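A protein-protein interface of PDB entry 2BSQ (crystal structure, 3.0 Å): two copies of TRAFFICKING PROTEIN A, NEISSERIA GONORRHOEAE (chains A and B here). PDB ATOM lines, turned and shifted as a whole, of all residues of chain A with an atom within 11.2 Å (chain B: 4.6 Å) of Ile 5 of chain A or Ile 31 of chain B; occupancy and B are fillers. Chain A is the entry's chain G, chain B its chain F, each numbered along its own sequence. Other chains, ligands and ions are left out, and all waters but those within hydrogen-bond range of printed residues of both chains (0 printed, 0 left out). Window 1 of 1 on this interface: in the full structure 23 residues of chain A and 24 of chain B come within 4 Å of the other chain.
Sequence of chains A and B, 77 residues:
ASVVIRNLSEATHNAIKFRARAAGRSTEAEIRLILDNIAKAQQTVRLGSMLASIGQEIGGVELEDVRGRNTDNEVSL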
ATOM      1  N   ALA A   1       9.181  19.877  30.582  1.00  0.00           N
ATOM      2  CA  ALA A   1       9.053  21.190  31.259  1.00  0.00           C
ATOM      3  C   ALA A   1       8.152  22.116  30.469  1.00  0.00           C
ATOM      4  O   ALA A   1       7.545  21.720  29.478  1.00  0.00           O
ATOM      5  CB  ALA A   1      10.420  21.831  31.416  1.00  0.00           C
ATOM      6  N   SER A   2       8.081  23.359  30.929  1.00  0.00           N
ATOM      7  CA  SER A   2       7.284  24.400  30.297  1.00  0.00           C
ATOM      8  C   SER A   2       8.203  25.590  30.090  1.00  0.00           C
ATOM      9  O   SER A   2       9.249  25.694  30.731  1.00  0.00           O
ATOM     10  CB  SER A   2       6.142  24.837  31.217  1.00  0.00           C
ATOM     11  OG  SER A   2       5.206  23.806  31.446  1.00  0.00           O
ATOM     12  N   VAL A   3       7.825  26.483  29.190  1.00  0.00           N
ATOM     13  CA  VAL A   3       8.608  27.689  28.933  1.00  0.00           C
ATOM     14  C   VAL A   3       7.665  28.637  28.245  1.00  0.00           C
ATOM     15  O   VAL A   3       6.844  28.209  27.438  1.00  0.00           O
ATOM     16  CB  VAL A   3       9.781  27.465  27.958  1.00  0.00           C
ATOM     17  CG1 VAL A   3      10.779  26.497  28.532  1.00  0.00           C
ATOM     18  CG2 VAL A   3       9.258  26.952  26.648  1.00  0.00           C
ATOM     19  N   VAL A   4       7.752  29.919  28.570  1.00  0.00           N
ATOM     20  CA  VAL A   4       6.899  30.882  27.900  1.00  0.00           C
ATOM     21  C   VAL A   4       7.808  31.798  27.096  1.00  0.00           C
ATOM     22  O   VAL A   4       8.806  32.315  27.596  1.00  0.00           O
ATOM     23  CB  VAL A   4       6.063  31.706  28.890  1.00  0.00           C
ATOM     24  CG1 VAL A   4       6.969  32.424  29.861  1.00  0.00           C
ATOM     25  CG2 VAL A   4       5.202  32.702  28.135  1.00  0.00           C
ATOM     26  N   ILE A   5       7.483  31.960  25.829  1.00  0.00           N
ATOM     27  CA  ILE A   5       8.282  32.802  24.983  1.00  0.00           C
ATOM     28  C   ILE A   5       7.541  34.110  24.801  1.00  0.00           C
ATOM     29  O   ILE A   5       6.586  34.208  24.033  1.00  0.00           O
ATOM     30  CB  ILE A   5       8.573  32.096  23.631  1.00  0.00           C
ATOM     31  CG1 ILE A   5       9.733  31.114  23.806  1.00  0.00           C
ATOM     32  CG2 ILE A   5       8.972  33.100  22.573  1.00  0.00           C
ATOM     33  CD1 ILE A   5       9.609  30.212  25.002  1.00  0.00           C
ATOM     34  N   ARG A   6       7.977  35.116  25.547  1.00  0.00           N
ATOM     35  CA  ARG A   6       7.363  36.428  25.472  1.00  0.00           C
ATOM     36  C   ARG A   6       8.089  37.288  24.456  1.00  0.00           C
ATOM     37  O   ARG A   6       9.264  37.071  24.150  1.00  0.00           O
ATOM     38  CB  ARG A   6       7.374  37.090  26.853  1.00  0.00           C
ATOM     39  CG  ARG A   6       6.314  36.527  27.803  1.00  0.00           C
ATOM     40  CD  ARG A   6       6.742  36.587  29.257  1.00  0.00           C
ATOM     41  NE  ARG A   6       7.916  35.756  29.510  1.00  0.00           N
ATOM     42  CZ  ARG A   6       8.278  35.328  30.716  1.00  0.00           C
ATOM     43  NH1 ARG A   6       7.552  35.647  31.783  1.00  0.00           N
ATOM     44  NH2 ARG A   6       9.375  34.589  30.861  1.00  0.00           N
ATOM     45  N   ASN A   7       7.375  38.270  23.929  1.00  0.00           N
ATOM     46  CA  ASN A   7       7.930  39.166  22.931  1.00  0.00           C
ATOM     47  C   ASN A   7       8.412  38.406  21.714  1.00  0.00           C
ATOM     48  O   ASN A   7       9.583  38.483  21.355  1.00  0.00           O
ATOM     49  CB  ASN A   7       9.079  39.977  23.516  1.00  0.00           C
ATOM     50  CG  ASN A   7       8.607  40.978  24.546  1.00  0.00           C
ATOM     51  OD1 ASN A   7       7.659  41.726  24.299  1.00  0.00           O
ATOM     52  ND2 ASN A   7       9.266  41.005  25.707  1.00  0.00           N
ATOM     53  N   LEU A   8       7.502  37.660  21.091  1.00  0.00           N
ATOM     54  CA  LEU A   8       7.804  36.905  19.883  1.00  0.00           C
ATOM     55  C   LEU A   8       7.134  37.729  18.784  1.00  0.00           C
ATOM     56  O   LEU A   8       5.926  37.922  18.830  1.00  0.00           O
ATOM     57  CB  LEU A   8       7.165  35.521  19.966  1.00  0.00           C
ATOM     58  CG  LEU A   8       7.921  34.333  19.371  1.00  0.00           C
ATOM     59  CD1 LEU A   8       7.073  33.072  19.470  1.00  0.00           C
ATOM     60  CD2 LEU A   8       8.248  34.610  17.940  1.00  0.00           C
ATOM     61  N   SER A   9       7.894  38.240  17.817  1.00  0.00           N
ATOM     62  CA  SER A   9       7.294  39.054  16.754  1.00  0.00           C
ATOM     63  C   SER A   9       6.141  38.340  16.048  1.00  0.00           C
ATOM     64  O   SER A   9       6.239  37.157  15.721  1.00  0.00           O
ATOM     65  CB  SER A   9       8.337  39.434  15.716  1.00  0.00           C
ATOM     66  OG  SER A   9       8.716  38.298  14.963  1.00  0.00           O
ATOM     67  N   GLU A  10       5.054  39.066  15.801  1.00  0.00           N
ATOM     68  CA  GLU A  10       3.895  38.485  15.137  1.00  0.00           C
ATOM     69  C   GLU A  10       4.309  37.855  13.803  1.00  0.00           C
ATOM     70  O   GLU A  10       3.710  36.866  13.359  1.00  0.00           O
ATOM     71  CB  GLU A  10       2.814  39.547  14.892  1.00  0.00           C
ATOM     72  CG  GLU A  10       2.362  40.336  16.130  1.00  0.00           C
ATOM     73  CD  GLU A  10       1.591  39.513  17.175  1.00  0.00           C
ATOM     74  OE1 GLU A  10       0.683  38.738  16.774  1.00  0.00           O
ATOM     75  OE2 GLU A  10       1.879  39.664  18.397  1.00  0.00           O
ATOM     76  N   THR A  12       7.282  36.284  12.943  1.00  0.00           N
ATOM     77  CA  THR A  12       7.805  34.969  13.256  1.00  0.00           C
ATOM     78  C   THR A  12       6.673  34.080  13.706  1.00  0.00           C
ATOM     79  O   THR A  12       6.559  32.930  13.290  1.00  0.00           O
ATOM     80  CB  THR A  12       8.794  35.032  14.404  1.00  0.00           C
ATOM     81  OG1 THR A  12       9.813  35.988  14.092  1.00  0.00           O
ATOM     82  CG2 THR A  12       9.416  33.652  14.656  1.00  0.00           C
ATOM     83  N   HIS A  13       5.840  34.632  14.577  1.00  0.00           N
ATOM     84  CA  HIS A  13       4.720  33.897  15.111  1.00  0.00           C
ATOM     85  C   HIS A  13       3.850  33.374  13.992  1.00  0.00           C
ATOM     86  O   HIS A  13       3.570  32.181  13.939  1.00  0.00           O
ATOM     87  CB  HIS A  13       3.892  34.781  16.023  1.00  0.00           C
ATOM     88  CG  HIS A  13       2.886  34.024  16.827  1.00  0.00           C
ATOM     89  ND1 HIS A  13       1.583  34.446  16.981  1.00  0.00           N
ATOM     90  CD2 HIS A  13       2.996  32.880  17.541  1.00  0.00           C
ATOM     91  CE1 HIS A  13       0.935  33.596  17.756  1.00  0.00           C
ATOM     92  NE2 HIS A  13       1.771  32.636  18.110  1.00  0.00           N
ATOM     93  N   ASN A  14       3.423  34.250  13.087  1.00  0.00           N
ATOM     94  CA  ASN A  14       2.577  33.803  11.988  1.00  0.00           C
ATOM     95  C   ASN A  14       3.301  32.792  11.125  1.00  0.00           C
ATOM     96  O   ASN A  14       2.699  31.852  10.611  1.00  0.00           O
ATOM     97  CB  ASN A  14       2.117  34.983  11.141  1.00  0.00           C
ATOM     98  CG  ASN A  14       1.137  35.873  11.883  1.00  0.00           C
ATOM     99  OD1 ASN A  14       0.583  35.469  12.917  1.00  0.00           O
ATOM    100  ND2 ASN A  14       0.908  37.087  11.359  1.00  0.00           N
ATOM    101  N   ILE A  16       5.365  30.584  12.131  1.00  0.00           N
ATOM    102  CA  ILE A  16       5.310  29.312  12.822  1.00  0.00           C
ATOM    103  C   ILE A  16       3.922  28.726  12.821  1.00  0.00           C
ATOM    104  O   ILE A  16       3.776  27.505  12.774  1.00  0.00           O
ATOM    105  CB  ILE A  16       5.833  29.433  14.269  1.00  0.00           C
ATOM    106  CG1 ILE A  16       7.220  30.097  14.271  1.00  0.00           C
ATOM    107  CG2 ILE A  16       5.936  28.054  14.900  1.00  0.00           C
ATOM    108  CD1 ILE A  16       8.320  29.273  13.657  1.00  0.00           C
ATOM    109  N   THR A  27       0.630  24.599  16.867  1.00  0.00           N
ATOM    110  CA  THR A  27       1.841  25.373  16.985  1.00  0.00           C
ATOM    111  C   THR A  27       2.673  24.881  18.143  1.00  0.00           C
ATOM    112  O   THR A  27       3.894  24.808  18.049  1.00  0.00           O
ATOM    113  CB  THR A  27       1.560  26.827  17.201  1.00  0.00           C
ATOM    114  OG1 THR A  27       0.527  27.247  16.311  1.00  0.00           O
ATOM    115  CG2 THR A  27       2.797  27.614  16.911  1.00  0.00           C
ATOM    116  N   GLU A  28       2.028  24.533  19.243  1.00  0.00           N
ATOM    117  CA  GLU A  28       2.805  24.065  20.367  1.00  0.00           C
ATOM    118  C   GLU A  28       3.436  22.743  19.981  1.00  0.00           C
ATOM    119  O   GLU A  28       4.506  22.400  20.457  1.00  0.00           O
ATOM    120  CB  GLU A  28       1.933  23.915  21.611  1.00  0.00           C
ATOM    121  CG  GLU A  28       2.721  23.644  22.887  1.00  0.00           C
ATOM    122  CD  GLU A  28       1.868  23.754  24.149  1.00  0.00           C
ATOM    123  OE1 GLU A  28       2.356  23.384  25.242  1.00  0.00           O
ATOM    124  OE2 GLU A  28       0.708  24.218  24.049  1.00  0.00           O
ATOM    125  N   GLU A  30       4.405  22.015  16.939  1.00  0.00           N
ATOM    126  CA  GLU A  30       5.447  22.376  15.987  1.00  0.00           C
ATOM    127  C   GLU A  30       6.702  22.866  16.688  1.00  0.00           C
ATOM    128  O   GLU A  30       7.807  22.488  16.302  1.00  0.00           O
ATOM    129  CB  GLU A  30       4.969  23.481  15.041  1.00  0.00           C
ATOM    130  CG  GLU A  30       4.790  23.032  13.610  1.00  0.00           C
ATOM    131  CD  GLU A  30       6.033  22.381  13.037  1.00  0.00           C
ATOM    132  OE1 GLU A  30       7.073  23.074  12.915  1.00  0.00           O
ATOM    133  OE2 GLU A  30       5.967  21.173  12.709  1.00  0.00           O
ATOM    134  N   ILE A  31       6.543  23.713  17.705  1.00  0.00           N
ATOM    135  CA  ILE A  31       7.708  24.248  18.398  1.00  0.00           C
ATOM    136  C   ILE A  31       8.401  23.130  19.154  1.00  0.00           C
ATOM    137  O   ILE A  31       9.637  23.007  19.153  1.00  0.00           O
ATOM    138  CB  ILE A  31       7.321  25.393  19.362  1.00  0.00           C
ATOM    139  CG1 ILE A  31       6.902  26.619  18.549  1.00  0.00           C
ATOM    140  CG2 ILE A  31       8.512  25.769  20.237  1.00  0.00           C
ATOM    141  CD1 ILE A  31       6.292  27.753  19.352  1.00  0.00           C
ATOM    142  N   ARG A  32       7.583  22.307  19.786  1.00  0.00           N
ATOM    143  CA  ARG A  32       8.065  21.183  20.547  1.00  0.00           C
ATOM    144  C   ARG A  32       8.951  20.358  19.597  1.00  0.00           C
ATOM    145  O   ARG A  32      10.053  19.949  19.946  1.00  0.00           O
ATOM    146  CB  ARG A  32       6.836  20.417  21.031  1.00  0.00           C
ATOM    147  CG  ARG A  32       7.045  19.251  21.961  1.00  0.00           C
ATOM    148  CD  ARG A  32       5.666  18.696  22.376  1.00  0.00           C
ATOM    149  NE  ARG A  32       4.910  19.705  23.108  1.00  0.00           N
ATOM    150  CZ  ARG A  32       3.599  19.895  23.003  1.00  0.00           C
ATOM    151  NH1 ARG A  32       2.865  19.142  22.192  1.00  0.00           N
ATOM    152  NH2 ARG A  32       3.017  20.857  23.705  1.00  0.00           N
ATOM    153  N   LEU A  33       8.487  20.167  18.370  1.00  0.00           N
ATOM    154  CA  LEU A  33       9.234  19.383  17.389  1.00  0.00           C
ATOM    155  C   LEU A  33      10.501  20.092  16.934  1.00  0.00           C
ATOM    156  O   LEU A  33      11.585  19.521  16.967  1.00  0.00           O
ATOM    157  CB  LEU A  33       8.358  19.086  16.165  1.00  0.00           C
ATOM    158  CG  LEU A  33       8.596  17.728  15.499  1.00  0.00           C
ATOM    159  CD1 LEU A  33       7.671  17.563  14.312  1.00  0.00           C
ATOM    160  CD2 LEU A  33      10.038  17.620  15.057  1.00  0.00           C
ATOM    161  N   ILE A  34      10.345  21.331  16.490  1.00  0.00           N
ATOM    162  CA  ILE A  34      11.460  22.124  16.026  1.00  0.00           C
ATOM    163  C   ILE A  34      12.577  22.065  17.049  1.00  0.00           C
ATOM    164  O   ILE A  34      13.743  21.839  16.702  1.00  0.00           O
ATOM    165  CB  ILE A  34      11.033  23.577  15.815  1.00  0.00           C
ATOM    166  CG1 ILE A  34      10.077  23.658  14.616  1.00  0.00           C
ATOM    167  CG2 ILE A  34      12.257  24.454  15.632  1.00  0.00           C
ATOM    168  CD1 ILE A  34       9.614  25.056  14.259  1.00  0.00           C
ATOM    169  N   LEU A  35      12.221  22.269  18.314  1.00  0.00           N
ATOM    170  CA  LEU A  35      13.200  22.216  19.384  1.00  0.00           C
ATOM    171  C   LEU A  35      13.763  20.807  19.506  1.00  0.00           C
ATOM    172  O   LEU A  35      14.973  20.628  19.600  1.00  0.00           O
ATOM    173  CB  LEU A  35      12.560  22.630  20.698  1.00  0.00           C
ATOM    174  CG  LEU A  35      12.234  24.117  20.789  1.00  0.00           C
ATOM    175  CD1 LEU A  35      11.530  24.412  22.099  1.00  0.00           C
ATOM    176  CD2 LEU A  35      13.514  24.926  20.673  1.00  0.00           C
ATOM    177  N   ASP A  36      12.888  19.807  19.498  1.00  0.00           N
ATOM    178  CA  ASP A  36      13.334  18.430  19.595  1.00  0.00           C
ATOM    179  C   ASP A  36      14.417  18.102  18.581  1.00  0.00           C
ATOM    180  O   ASP A  36      15.462  17.577  18.927  1.00  0.00           O
ATOM    181  CB  ASP A  36      12.170  17.463  19.399  1.00  0.00           C
ATOM    182  CG  ASP A  36      11.227  17.426  20.596  1.00  0.00           C
ATOM    183  OD1 ASP A  36      11.703  17.437  21.762  1.00  0.00           O
ATOM    184  OD2 ASP A  36       9.994  17.368  20.373  1.00  0.00           O
ATOM    185  N   ILE A  38      16.418  20.002  17.037  1.00  0.00           N
ATOM    186  CA  ILE A  38      17.641  20.708  17.352  1.00  0.00           C
ATOM    187  C   ILE A  38      18.354  19.979  18.472  1.00  0.00           C
ATOM    188  O   ILE A  38      19.551  19.695  18.392  1.00  0.00           O
ATOM    189  CB  ILE A  38      17.333  22.130  17.774  1.00  0.00           C
ATOM    190  CG1 ILE A  38      17.057  22.968  16.525  1.00  0.00           C
ATOM    191  CG2 ILE A  38      18.457  22.670  18.632  1.00  0.00           C
ATOM    192  CD1 ILE A  38      16.431  24.292  16.821  1.00  0.00           C
ATOM    193  N   ALA A  39      17.599  19.668  19.516  1.00  0.00           N
ATOM    194  CA  ALA A  39      18.147  18.969  20.665  1.00  0.00           C
ATOM    195  C   ALA A  39      18.760  17.648  20.228  1.00  0.00           C
ATOM    196  O   ALA A  39      19.845  17.283  20.672  1.00  0.00           O
ATOM    197  CB  ALA A  39      17.057  18.725  21.698  1.00  0.00           C
ATOM    198  N   ALA B   1       4.249  38.764  20.733  1.00  0.00           N
ATOM    199  CA  ALA B   1       3.246  37.707  21.048  1.00  0.00           C
ATOM    200  C   ALA B   1       3.826  36.708  22.041  1.00  0.00           C
ATOM    201  O   ALA B   1       5.040  36.506  22.092  1.00  0.00           O
ATOM    202  CB  ALA B   1       2.816  36.982  19.772  1.00  0.00           C
ATOM    203  N   SER B   2       2.959  36.089  22.831  1.00  0.00           N
ATOM    204  CA  SER B   2       3.394  35.112  23.808  1.00  0.00           C
ATOM    205  C   SER B   2       3.068  33.721  23.317  1.00  0.00           C
ATOM    206  O   SER B   2       2.128  33.534  22.566  1.00  0.00           O
ATOM    207  CB  SER B   2       2.680  35.342  25.134  1.00  0.00           C
ATOM    208  OG  SER B   2       3.254  36.401  25.867  1.00  0.00           O
ATOM    209  N   VAL B   3       3.842  32.738  23.744  1.00  0.00           N
ATOM    210  CA  VAL B   3       3.595  31.356  23.354  1.00  0.00           C
ATOM    211  C   VAL B   3       4.103  30.453  24.468  1.00  0.00           C
ATOM    212  O   VAL B   3       5.234  30.621  24.934  1.00  0.00           O
ATOM    213  CB  VAL B   3       4.315  31.004  22.035  1.00  0.00           C
ATOM    214  CG1 VAL B   3       4.414  29.497  21.868  1.00  0.00           C
ATOM    215  CG2 VAL B   3       3.550  31.586  20.873  1.00  0.00           C
ATOM    216  N   ILE B  16      18.533  22.803  24.694  1.00  0.00           N
ATOM    217  CA  ILE B  16      18.311  24.183  24.292  1.00  0.00           C
ATOM    218  C   ILE B  16      18.972  25.103  25.322  1.00  0.00           C
ATOM    219  O   ILE B  16      19.666  26.062  24.979  1.00  0.00           O
ATOM    220  CB  ILE B  16      16.793  24.491  24.195  1.00  0.00           C
ATOM    221  CG1 ILE B  16      16.134  23.508  23.234  1.00  0.00           C
ATOM    222  CG2 ILE B  16      16.552  25.899  23.675  1.00  0.00           C
ATOM    223  CD1 ILE B  16      16.682  23.565  21.830  1.00  0.00           C
ATOM    224  N   THR B  27      17.760  31.229  27.960  1.00  0.00           N
ATOM    225  CA  THR B  27      17.077  30.220  27.175  1.00  0.00           C
ATOM    226  C   THR B  27      15.939  30.836  26.387  1.00  0.00           C
ATOM    227  O   THR B  27      15.781  30.576  25.200  1.00  0.00           O
ATOM    228  CB  THR B  27      16.529  29.094  28.021  1.00  0.00           C
ATOM    229  OG1 THR B  27      17.617  28.404  28.643  1.00  0.00           O
ATOM    230  CG2 THR B  27      15.772  28.117  27.148  1.00  0.00           C
ATOM    231  N   GLU B  28      15.152  31.681  27.025  1.00  0.00           N
ATOM    232  CA  GLU B  28      14.062  32.268  26.293  1.00  0.00           C
ATOM    233  C   GLU B  28      14.527  32.945  24.998  1.00  0.00           C
ATOM    234  O   GLU B  28      13.935  32.743  23.944  1.00  0.00           O
ATOM    235  CB  GLU B  28      13.305  33.252  27.175  1.00  0.00           C
ATOM    236  CG  GLU B  28      12.136  33.877  26.447  1.00  0.00           C
ATOM    237  CD  GLU B  28      11.204  34.630  27.358  1.00  0.00           C
ATOM    238  OE1 GLU B  28      10.285  35.291  26.823  1.00  0.00           O
ATOM    239  OE2 GLU B  28      11.383  34.553  28.599  1.00  0.00           O
ATOM    240  N   ALA B  29      15.591  33.737  25.058  1.00  0.00           N
ATOM    241  CA  ALA B  29      16.066  34.423  23.859  1.00  0.00           C
ATOM    242  C   ALA B  29      16.504  33.429  22.795  1.00  0.00           C
ATOM    243  O   ALA B  29      16.314  33.657  21.596  1.00  0.00           O
ATOM    244  CB  ALA B  29      17.202  35.321  24.205  1.00  0.00           C
ATOM    245  N   GLU B  30      17.101  32.329  23.245  1.00  0.00           N
ATOM    246  CA  GLU B  30      17.561  31.265  22.356  1.00  0.00           C
ATOM    247  C   GLU B  30      16.393  30.752  21.496  1.00  0.00           C
ATOM    248  O   GLU B  30      16.448  30.791  20.274  1.00  0.00           O
ATOM    249  CB  GLU B  30      18.148  30.126  23.203  1.00  0.00           C
ATOM    250  CG  GLU B  30      18.667  28.928  22.435  1.00  0.00           C
ATOM    251  CD  GLU B  30      19.719  29.294  21.401  1.00  0.00           C
ATOM    252  OE1 GLU B  30      20.490  30.253  21.645  1.00  0.00           O
ATOM    253  OE2 GLU B  30      19.782  28.609  20.348  1.00  0.00           O
ATOM    254  N   ILE B  31      15.335  30.282  22.145  1.00  0.00           N
ATOM    255  CA  ILE B  31      14.170  29.764  21.441  1.00  0.00           C
ATOM    256  C   ILE B  31      13.613  30.816  20.497  1.00  0.00           C
ATOM    257  O   ILE B  31      13.232  30.531  19.361  1.00  0.00           O
ATOM    258  CB  ILE B  31      13.061  29.342  22.434  1.00  0.00           C
ATOM    259  CG1 ILE B  31      13.571  28.198  23.303  1.00  0.00           C
ATOM    260  CG2 ILE B  31      11.808  28.917  21.686  1.00  0.00           C
ATOM    261  CD1 ILE B  31      12.620  27.781  24.376  1.00  0.00           C
ATOM    262  N   ARG B  32      13.571  32.040  20.984  1.00  0.00           N
ATOM    263  CA  ARG B  32      13.066  33.166  20.209  1.00  0.00           C
ATOM    264  C   ARG B  32      13.895  33.317  18.911  1.00  0.00           C
ATOM    265  O   ARG B  32      13.358  33.585  17.833  1.00  0.00           O
ATOM    266  CB  ARG B  32      13.156  34.416  21.092  1.00  0.00           C
ATOM    267  CG  ARG B  32      12.347  35.588  20.658  1.00  0.00           C
ATOM    268  CD  ARG B  32      12.703  36.774  21.541  1.00  0.00           C
ATOM    269  NE  ARG B  32      12.119  36.679  22.878  1.00  0.00           N
ATOM    270  CZ  ARG B  32      12.802  36.860  24.008  1.00  0.00           C
ATOM    271  NH1 ARG B  32      14.103  37.133  23.965  1.00  0.00           N
ATOM    272  NH2 ARG B  32      12.178  36.804  25.183  1.00  0.00           N
ATOM    273  N   LEU B  33      15.204  33.124  19.021  1.00  0.00           N
ATOM    274  CA  LEU B  33      16.077  33.240  17.868  1.00  0.00           C
ATOM    275  C   LEU B  33      15.820  32.082  16.932  1.00  0.00           C
ATOM    276  O   LEU B  33      15.656  32.252  15.734  1.00  0.00           O
ATOM    277  CB  LEU B  33      17.529  33.215  18.308  1.00  0.00           C
ATOM    278  CG  LEU B  33      18.528  33.207  17.159  1.00  0.00           C
ATOM    279  CD1 LEU B  33      18.454  34.535  16.453  1.00  0.00           C
ATOM    280  CD2 LEU B  33      19.936  32.924  17.688  1.00  0.00           C
ATOM    281  N   ILE B  34      15.796  30.888  17.491  1.00  0.00           N
ATOM    282  CA  ILE B  34      15.547  29.703  16.704  1.00  0.00           C
ATOM    283  C   ILE B  34      14.307  29.905  15.862  1.00  0.00           C
ATOM    284  O   ILE B  34      14.387  29.923  14.642  1.00  0.00           O
ATOM    285  CB  ILE B  34      15.387  28.498  17.608  1.00  0.00           C
ATOM    286  CG1 ILE B  34      16.740  28.200  18.263  1.00  0.00           C
ATOM    287  CG2 ILE B  34      14.850  27.344  16.824  1.00  0.00           C
ATOM    288  CD1 ILE B  34      16.757  26.975  19.125  1.00  0.00           C
ATOM    289  N   LEU B  35      13.163  30.082  16.505  1.00  0.00           N
ATOM    290  CA  LEU B  35      11.925  30.299  15.771  1.00  0.00           C
ATOM    291  C   LEU B  35      12.088  31.421  14.752  1.00  0.00           C
ATOM    292  O   LEU B  35      11.494  31.379  13.679  1.00  0.00           O
ATOM    293  CB  LEU B  35      10.792  30.623  16.741  1.00  0.00           C
ATOM    294  CG  LEU B  35       9.964  29.428  17.228  1.00  0.00           C
ATOM    295  CD1 LEU B  35      10.786  28.157  17.274  1.00  0.00           C
ATOM    296  CD2 LEU B  35       9.385  29.752  18.580  1.00  0.00           C
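Printed residues of chain B that touch a printed residue of chain A: Ala 1, Ser 2, Val 3, Ile 16, Glu 28, Ile 31, Arg 32, Ile 34 and Leu 35.
Hydrophobic or aromatic side chains of chain B within 4 Å of the printed part of chain A: Ala 1, Val 3, Ile 16, Ile 31, Ile 34 and Leu 35.
Among the printed residues, 25 pairs touch across the chains.
Of the printed residues of chain B, Leu 8 of chain A touches Ala 1.
Printed residues of chain B within 4 Å of His 13 of chain A: Ala 1 and Val 3.
Arg 32 of chain A touches none of the printed residues of chain B.
Printed residues of chain B within 4 Å of Ile 38 of chain A: Ile 16 (3.8 Å) and Ile 34 (3.4 Å).
Glu 28 of chain B touches just these residues of chain A: Val 4 (3.3 Å), Ile 5 (3.6 Å) and Arg 6 (2.6 Å).
Ala 29 of chain B touches none of the printed residues of chain A.
No residue of chain A comes within 4 Å of Glu 30 of chain B.
Ile 31 of chain B touches one residue of chain A.
Of chain A, only Thr 12 (3.2 Å), Ile 16 (3.8 Å) and Ile 31 (3.8 Å) come within 4 Å of Leu 35 of chain B.
The nearest printed residue of chain B that does not touch Ile 38 of chain A is Glu 30 of chain B (6.3 Å).
Val 3 of chain B touches its own counterpart, Val 3 of chain A.
Ile 16 of chain A touches Leu 35 of chain B, and with the chains exchanged Leu 35 of chain A touches Ile 16 of chain B.
Ile 31 of chain A touches Val 3 of chain B, but with the chains exchanged Val 3 of chain A does not touch Ile 31 of chain B (4.1 Å).
Positions printed for both chains: 1, 2, 3, 16, 27, 28, 30, 31, 32, 33, 34 and 35.
The backbone NH (N) of Asn 7 of chain A is in hydrogen-bond range of the backbone carbonyl oxygen (O) of Ala 1 of chain B (3.5 Å).
The backbone NH (N) of Ala 1 of chain B is in hydrogen-bond range of the backbone carbonyl oxygen (O) of Leu 8 of chain A (2.7 Å).
The backbone NH (N) of Ala 1 of chain B lies close to the side-chain carboxylate (OE2) of Glu 10 of chain A (3.4 Å).
O of Val 3 of chain B is in hydrogen-bond range of N of Ile 5 of chain A, 2.8 Å away.
OE2 of Glu 28 of chain B is in salt-bridge range of NH2 of Arg 6 of chain A.
O of Arg 6 of chain A is in hydrogen-bond range of NH2 of Arg 32 of chain B, 3.1 Å away.
The backbone carbonyl oxygen (O) of Asn 7 of chain A is in hydrogen-bond range of the guanidinium group (NE) of Arg 32 of chain B, at 3.5 Å.
The backbone carbonyl oxygen (O) of Val 4 of chain A sits close to the side-chain carboxylate (OE1) of Glu 28 of chain B, 3.4 Å away.
The backbone carbonyl oxygen of Ile 5 of chain A lies close to the backbone carbonyl oxygen of Ala 1 of chain B (3.4 Å).
Among the printed residues, pairs that only touch across the chains: Val 3 of chain A with Val 3 of chain B (3.8 Å), Val 4 of chain A with Val 3 of chain B (3.4 Å), Ile 5 of chain A with Ser 2 of chain B (3.3 Å), Ile 5 of chain A with Glu 28 of chain B (3.6 Å), Ile 5 of chain A with Ile 31 of chain B (3.7 Å), Arg 6 of chain A with Ala 1 of chain B (3.9 Å), Arg 6 of chain A with Ser 2 of chain B (3.6 Å), Thr 12 of chain A with Leu 35 of chain B (3.2 Å), His 13 of chain A with Ala 1 of chain B (3.97 Å), His 13 of chain A with Val 3 of chain B (3.4 Å), Ile 16 of chain A with Leu 35 of chain B (3.8 Å), Ile 31 of chain A with Val 3 of chain B (3.6 Å), Ile 31 of chain A with Leu 35 of chain B (3.8 Å), Leu 35 of chain A with Ile 16 of chain B (3.6 Å), Ile 38 of chain A with Ile 16 of chain B (3.8 Å) and Ile 38 of chain A with Ile 34 of chain B (3.4 Å).
The side-chain carboxylate (OE1) of Glu 28 of chain B lies within salt-bridge range of the guanidinium group (NH2) of Arg 32 of chain B, 2.9 Å away.
The side-chain hydroxyl (OG) of Ser 9 of chain A sits at hydrogen-bond distance from the side-chain hydroxyl (OG1) of Thr 12 of chain A.
O of Glu 10 of chain A lies close to ND2 of Asn 14 of chain A (3.4 Å).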
